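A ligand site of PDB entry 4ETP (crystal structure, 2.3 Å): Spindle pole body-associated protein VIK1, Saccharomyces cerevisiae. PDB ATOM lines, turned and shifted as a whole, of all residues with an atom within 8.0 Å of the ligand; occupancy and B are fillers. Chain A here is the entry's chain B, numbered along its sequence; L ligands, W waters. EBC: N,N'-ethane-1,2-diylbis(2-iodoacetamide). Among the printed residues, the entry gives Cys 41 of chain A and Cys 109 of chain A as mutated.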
ATOM      1  N   ASN A  34     -19.381  -2.754  -3.049  1.00  0.00           N
ATOM      2  CA  ASN A  34     -20.146  -3.224  -4.210  1.00  0.00           C
ATOM      3  C   ASN A  34     -21.346  -2.358  -4.546  1.00  0.00           C
ATOM      4  O   ASN A  34     -21.626  -2.102  -5.714  1.00  0.00           O
ATOM      5  CB  ASN A  34     -20.593  -4.683  -4.011  1.00  0.00           C
ATOM      6  CG  ASN A  34     -19.460  -5.685  -4.199  1.00  0.00           C
ATOM      7  OD1 ASN A  34     -18.401  -5.360  -4.723  1.00  0.00           O
ATOM      8  ND2 ASN A  34     -19.699  -6.915  -3.760  1.00  0.00           N
ATOM      9  N   THR A  36     -21.737   0.890  -3.741  1.00  0.00           N
ATOM     10  CA  THR A  36     -21.214   2.172  -4.202  1.00  0.00           C
ATOM     11  C   THR A  36     -20.632   2.063  -5.616  1.00  0.00           C
ATOM     12  O   THR A  36     -20.830   2.948  -6.438  1.00  0.00           O
ATOM     13  CB  THR A  36     -20.146   2.730  -3.238  1.00  0.00           C
ATOM     14  OG1 THR A  36     -20.597   2.567  -1.890  1.00  0.00           O
ATOM     15  CG2 THR A  36     -19.876   4.206  -3.511  1.00  0.00           C
ATOM     16  N   TYR A  37     -19.940   0.952  -5.872  1.00  0.00           N
ATOM     17  CA  TYR A  37     -19.362   0.669  -7.179  1.00  0.00           C
ATOM     18  C   TYR A  37     -20.445   0.552  -8.251  1.00  0.00           C
ATOM     19  O   TYR A  37     -20.313   1.110  -9.343  1.00  0.00           O
ATOM     20  CB  TYR A  37     -18.524  -0.616  -7.118  1.00  0.00           C
ATOM     21  CG  TYR A  37     -17.818  -1.000  -8.395  1.00  0.00           C
ATOM     22  CD1 TYR A  37     -16.678  -0.324  -8.836  1.00  0.00           C
ATOM     23  CD2 TYR A  37     -18.282  -2.065  -9.170  1.00  0.00           C
ATOM     24  CE1 TYR A  37     -16.027  -0.686  -9.997  1.00  0.00           C
ATOM     25  CE2 TYR A  37     -17.641  -2.433 -10.343  1.00  0.00           C
ATOM     26  CZ  TYR A  37     -16.514  -1.743 -10.757  1.00  0.00           C
ATOM     27  OH  TYR A  37     -15.882  -2.113 -11.914  1.00  0.00           O
ATOM     28  N   ASN A  38     -21.523  -0.159  -7.924  1.00  0.00           N
ATOM     29  CA  ASN A  38     -22.663  -0.310  -8.839  1.00  0.00           C
ATOM     30  C   ASN A  38     -23.411   1.008  -9.060  1.00  0.00           C
ATOM     31  O   ASN A  38     -23.802   1.305 -10.190  1.00  0.00           O
ATOM     32  CB  ASN A  38     -23.619  -1.406  -8.354  1.00  0.00           C
ATOM     33  CG  ASN A  38     -23.038  -2.808  -8.528  1.00  0.00           C
ATOM     34  OD1 ASN A  38     -22.271  -3.063  -9.460  1.00  0.00           O
ATOM     35  ND2 ASN A  38     -23.406  -3.713  -7.635  1.00  0.00           N
ATOM     36  N   THR A  39     -23.578   1.788  -7.997  1.00  0.00           N
ATOM     37  CA  THR A  39     -24.197   3.115  -8.094  1.00  0.00           C
ATOM     38  C   THR A  39     -23.403   4.038  -9.045  1.00  0.00           C
ATOM     39  O   THR A  39     -23.987   4.680  -9.906  1.00  0.00           O
ATOM     40  CB  THR A  39     -24.374   3.774  -6.710  1.00  0.00           C
ATOM     41  OG1 THR A  39     -25.041   2.859  -5.838  1.00  0.00           O
ATOM     42  CG2 THR A  39     -25.206   5.054  -6.814  1.00  0.00           C
ATOM     43  N   VAL A  40     -22.078   4.065  -8.889  1.00  0.00           N
ATOM     44  CA  VAL A  40     -21.209   4.844  -9.775  1.00  0.00           C
ATOM     45  C   VAL A  40     -21.448   4.489 -11.246  1.00  0.00           C
ATOM     46  O   VAL A  40     -21.641   5.383 -12.078  1.00  0.00           O
ATOM     47  CB  VAL A  40     -19.713   4.701  -9.399  1.00  0.00           C
ATOM     48  CG1 VAL A  40     -18.806   5.261 -10.491  1.00  0.00           C
ATOM     49  CG2 VAL A  40     -19.424   5.403  -8.088  1.00  0.00           C
ATOM     50  N   CYS A  41     -21.458   3.189 -11.552  1.00  0.00           N
ATOM     51  CA  CYS A  41     -21.708   2.725 -12.921  1.00  0.00           C
ATOM     52  C   CYS A  41     -23.072   3.137 -13.442  1.00  0.00           C
ATOM     53  O   CYS A  41     -23.210   3.500 -14.608  1.00  0.00           O
ATOM     54  CB  CYS A  41     -21.561   1.208 -13.018  1.00  0.00           C
ATOM     55  SG  CYS A  41     -19.913   0.566 -12.659  1.00  0.00           S
ATOM     56  N   LYS A  42     -24.084   3.069 -12.575  1.00  0.00           N
ATOM     57  CA  LYS A  42     -25.444   3.459 -12.947  1.00  0.00           C
ATOM     58  C   LYS A  42     -25.565   4.964 -13.161  1.00  0.00           C
ATOM     59  O   LYS A  42     -26.192   5.411 -14.126  1.00  0.00           O
ATOM     60  CB  LYS A  42     -26.453   2.987 -11.893  1.00  0.00           C
ATOM     61  CG  LYS A  42     -26.695   1.481 -11.906  1.00  0.00           C
ATOM     62  CD  LYS A  42     -27.463   1.041 -10.662  1.00  0.00           C
ATOM     63  CE  LYS A  42     -27.678  -0.464 -10.649  1.00  0.00           C
ATOM     64  NZ  LYS A  42     -28.292  -0.911  -9.368  1.00  0.00           N
ATOM     65  N   LEU A  44     -23.130   7.074 -13.954  1.00  0.00           N
ATOM     66  CA  LEU A  44     -22.388   7.412 -15.160  1.00  0.00           C
ATOM     67  C   LEU A  44     -23.244   7.187 -16.405  1.00  0.00           C
ATOM     68  O   LEU A  44     -23.217   7.995 -17.342  1.00  0.00           O
ATOM     69  CB  LEU A  44     -21.082   6.610 -15.252  1.00  0.00           C
ATOM     70  CG  LEU A  44     -19.893   7.052 -14.392  1.00  0.00           C
ATOM     71  CD1 LEU A  44     -18.810   5.981 -14.410  1.00  0.00           C
ATOM     72  CD2 LEU A  44     -19.326   8.388 -14.839  1.00  0.00           C
ATOM     73  N   LEU A  45     -24.009   6.092 -16.400  1.00  0.00           N
ATOM     74  CA  LEU A  45     -24.940   5.800 -17.487  1.00  0.00           C
ATOM     75  C   LEU A  45     -26.102   6.787 -17.561  1.00  0.00           C
ATOM     76  O   LEU A  45     -26.595   7.082 -18.645  1.00  0.00           O
ATOM     77  CB  LEU A  45     -25.459   4.361 -17.394  1.00  0.00           C
ATOM     78  CG  LEU A  45     -24.546   3.319 -18.039  1.00  0.00           C
ATOM     79  CD1 LEU A  45     -24.867   1.939 -17.505  1.00  0.00           C
ATOM     80  CD2 LEU A  45     -24.650   3.334 -19.567  1.00  0.00           C
ATOM     81  N   LYS A 104      -8.839   3.618 -17.480  1.00  0.00           N
ATOM     82  CA  LYS A 104      -9.999   3.491 -16.595  1.00  0.00           C
ATOM     83  C   LYS A 104     -11.139   2.702 -17.239  1.00  0.00           C
ATOM     84  O   LYS A 104     -11.958   2.108 -16.540  1.00  0.00           O
ATOM     85  CB  LYS A 104     -10.491   4.873 -16.157  1.00  0.00           C
ATOM     86  CG  LYS A 104      -9.531   5.625 -15.251  1.00  0.00           C
ATOM     87  CD  LYS A 104     -10.052   7.010 -14.912  1.00  0.00           C
ATOM     88  CE  LYS A 104      -9.087   7.770 -14.015  1.00  0.00           C
ATOM     89  NZ  LYS A 104      -9.576   9.130 -13.682  1.00  0.00           N
ATOM     90  N   VAL A 105     -11.187   2.696 -18.565  1.00  0.00           N
ATOM     91  CA  VAL A 105     -12.264   2.048 -19.315  1.00  0.00           C
ATOM     92  C   VAL A 105     -11.726   0.980 -20.261  1.00  0.00           C
ATOM     93  O   VAL A 105     -10.996   1.273 -21.211  1.00  0.00           O
ATOM     94  CB  VAL A 105     -13.104   3.092 -20.110  1.00  0.00           C
ATOM     95  CG1 VAL A 105     -14.145   2.409 -20.987  1.00  0.00           C
ATOM     96  CG2 VAL A 105     -13.762   4.081 -19.159  1.00  0.00           C
ATOM     97  N   SER A 106     -12.109  -0.274 -19.999  1.00  0.00           N
ATOM     98  CA  SER A 106     -11.721  -1.392 -20.856  1.00  0.00           C
ATOM     99  C   SER A 106     -12.602  -1.464 -22.107  1.00  0.00           C
ATOM    100  O   SER A 106     -13.532  -0.678 -22.249  1.00  0.00           O
ATOM    101  CB  SER A 106     -11.793  -2.712 -20.082  1.00  0.00           C
ATOM    102  OG  SER A 106     -13.132  -3.080 -19.799  1.00  0.00           O
ATOM    103  N   GLU A 107     -12.293  -2.395 -23.001  1.00  0.00           N
ATOM    104  CA  GLU A 107     -13.071  -2.566 -24.234  1.00  0.00           C
ATOM    105  C   GLU A 107     -14.486  -3.056 -23.942  1.00  0.00           C
ATOM    106  O   GLU A 107     -15.438  -2.664 -24.627  1.00  0.00           O
ATOM    107  CB  GLU A 107     -12.360  -3.510 -25.206  1.00  0.00           C
ATOM    108  CG  GLU A 107     -11.165  -2.898 -25.929  1.00  0.00           C
ATOM    109  CD  GLU A 107      -9.864  -2.958 -25.132  1.00  0.00           C
ATOM    110  OE1 GLU A 107      -9.841  -3.593 -24.046  1.00  0.00           O
ATOM    111  OE2 GLU A 107      -8.862  -2.383 -25.598  1.00  0.00           O
ATOM    112  N   ASP A 108     -14.624  -3.902 -22.915  1.00  0.00           N
ATOM    113  CA  ASP A 108     -15.928  -4.378 -22.463  1.00  0.00           C
ATOM    114  C   ASP A 108     -16.725  -3.249 -21.817  1.00  0.00           C
ATOM    115  O   ASP A 108     -17.931  -3.128 -21.997  1.00  0.00           O
ATOM    116  CB  ASP A 108     -15.771  -5.522 -21.455  1.00  0.00           C
ATOM    117  CG  ASP A 108     -15.184  -6.770 -22.080  1.00  0.00           C
ATOM    118  OD1 ASP A 108     -15.613  -7.152 -23.188  1.00  0.00           O
ATOM    119  OD2 ASP A 108     -14.297  -7.382 -21.440  1.00  0.00           O
ATOM    120  N   CYS A 109     -16.014  -2.416 -21.048  1.00  0.00           N
ATOM    121  CA  CYS A 109     -16.598  -1.275 -20.366  1.00  0.00           C
ATOM    122  C   CYS A 109     -16.995  -0.187 -21.362  1.00  0.00           C
ATOM    123  O   CYS A 109     -17.997   0.498 -21.167  1.00  0.00           O
ATOM    124  CB  CYS A 109     -15.619  -0.717 -19.336  1.00  0.00           C
ATOM    125  SG  CYS A 109     -16.293   0.582 -18.271  1.00  0.00           S
ATOM    126  N   PHE A 110     -16.224  -0.036 -22.433  1.00  0.00           N
ATOM    127  CA  PHE A 110     -16.563   0.918 -23.502  1.00  0.00           C
ATOM    128  C   PHE A 110     -17.972   0.652 -24.036  1.00  0.00           C
ATOM    129  O   PHE A 110     -18.782   1.577 -24.159  1.00  0.00           O
ATOM    130  CB  PHE A 110     -15.548   0.890 -24.646  1.00  0.00           C
ATOM    131  CG  PHE A 110     -15.987   1.688 -25.857  1.00  0.00           C
ATOM    132  CD1 PHE A 110     -15.744   3.055 -25.932  1.00  0.00           C
ATOM    133  CD2 PHE A 110     -16.652   1.062 -26.909  1.00  0.00           C
ATOM    134  CE1 PHE A 110     -16.160   3.793 -27.038  1.00  0.00           C
ATOM    135  CE2 PHE A 110     -17.068   1.800 -28.015  1.00  0.00           C
ATOM    136  CZ  PHE A 110     -16.818   3.157 -28.075  1.00  0.00           C
ATOM    137  N   THR A 112     -20.514  -1.242 -22.690  1.00  0.00           N
ATOM    138  CA  THR A 112     -21.581  -1.182 -21.692  1.00  0.00           C
ATOM    139  C   THR A 112     -21.812   0.241 -21.185  1.00  0.00           C
ATOM    140  O   THR A 112     -22.964   0.654 -21.016  1.00  0.00           O
ATOM    141  CB  THR A 112     -21.317  -2.110 -20.483  1.00  0.00           C
ATOM    142  OG1 THR A 112     -20.148  -1.685 -19.777  1.00  0.00           O
ATOM    143  CG2 THR A 112     -21.169  -3.569 -20.925  1.00  0.00           C
ATOM    144  N   GLN A 113     -20.733   0.976 -20.952  1.00  0.00           N
ATOM    145  CA  GLN A 113     -20.806   2.306 -20.347  1.00  0.00           C
ATOM    146  C   GLN A 113     -20.918   3.449 -21.351  1.00  0.00           C
ATOM    147  O   GLN A 113     -21.716   4.372 -21.163  1.00  0.00           O
ATOM    148  CB  GLN A 113     -19.613   2.526 -19.400  1.00  0.00           C
ATOM    149  CG  GLN A 113     -19.488   3.942 -18.844  1.00  0.00           C
ATOM    150  CD  GLN A 113     -18.493   4.059 -17.707  1.00  0.00           C
ATOM    151  OE1 GLN A 113     -18.623   3.400 -16.667  1.00  0.00           O
ATOM    152  NE2 GLN A 113     -17.493   4.906 -17.887  1.00  0.00           N
ATOM    153  N   GLU A 114     -20.136   3.375 -22.429  1.00  0.00           N
ATOM    154  CA  GLU A 114     -19.983   4.506 -23.347  1.00  0.00           C
ATOM    155  C   GLU A 114     -20.744   4.339 -24.662  1.00  0.00           C
ATOM    156  O   GLU A 114     -20.964   5.317 -25.378  1.00  0.00           O
ATOM    157  CB  GLU A 114     -18.498   4.771 -23.622  1.00  0.00           C
ATOM    158  CG  GLU A 114     -17.607   4.836 -22.393  1.00  0.00           C
ATOM    159  CD  GLU A 114     -17.787   6.117 -21.580  1.00  0.00           C
ATOM    160  OE1 GLU A 114     -18.333   7.103 -22.116  1.00  0.00           O
ATOM    161  OE2 GLU A 114     -17.362   6.135 -20.407  1.00  0.00           O
HETATM  162  O10 EBC L   1     -20.349  -1.739 -14.798  1.00  0.00           O
HETATM  163  C2  EBC L   1     -19.672  -1.880 -13.790  1.00  0.00           C
HETATM  164  C1  EBC L   1     -20.045  -1.215 -12.491  1.00  0.00           C
HETATM  165  N3  EBC L   1     -18.562  -2.612 -13.747  1.00  0.00           N
HETATM  166  C4  EBC L   1     -18.121  -3.449 -14.846  1.00  0.00           C
HETATM  167  C5  EBC L   1     -16.876  -2.888 -15.534  1.00  0.00           C
HETATM  168  N6  EBC L   1     -17.170  -1.683 -16.288  1.00  0.00           N
HETATM  169  C7  EBC L   1     -16.862  -0.472 -15.832  1.00  0.00           C
HETATM  170  O9  EBC L   1     -17.424   0.034 -14.875  1.00  0.00           O
HETATM  171  C8  EBC L   1     -15.775   0.251 -16.574  1.00  0.00           C
HETATM  172  O   HOH W   1     -21.115  -0.237 -17.254  1.00  0.00           O
HETATM  173  O   HOH W   2     -18.746  -3.621 -18.192  1.00  0.00           O
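C1 of the ligand is covalently linked to SG of Cys 41. The side-chain sulfur (SG) of Cys 109 is bonded to a carbon (C8) of the ligand, 1.8 Å away. OH of Tyr 37 lies within hydrogen-bond range of N3 of the ligand (3.3 Å).
Water W1 lies within hydrogen-bond range of an oxygen (O10) of the ligand (3.0 Å) and the side-chain hydroxyl (OG1) of Thr 112 (3.1 Å). Water W2 bridges OG1 of Thr 112 (2.9 Å) and N6 of the ligand (3.1 Å).
OG of Ser 106 is in hydrogen-bond range of N of Cys 109 (3.2 Å). The side-chain hydroxyl (OG1) of Thr 112 lies within hydrogen-bond range of the backbone carbonyl oxygen (O) of Cys 109, at 3.4 Å. NE2 of Gln 113 is in hydrogen-bond range of OE2 of Glu 114 (2.8 Å).
Gln 113 touches the ligand.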
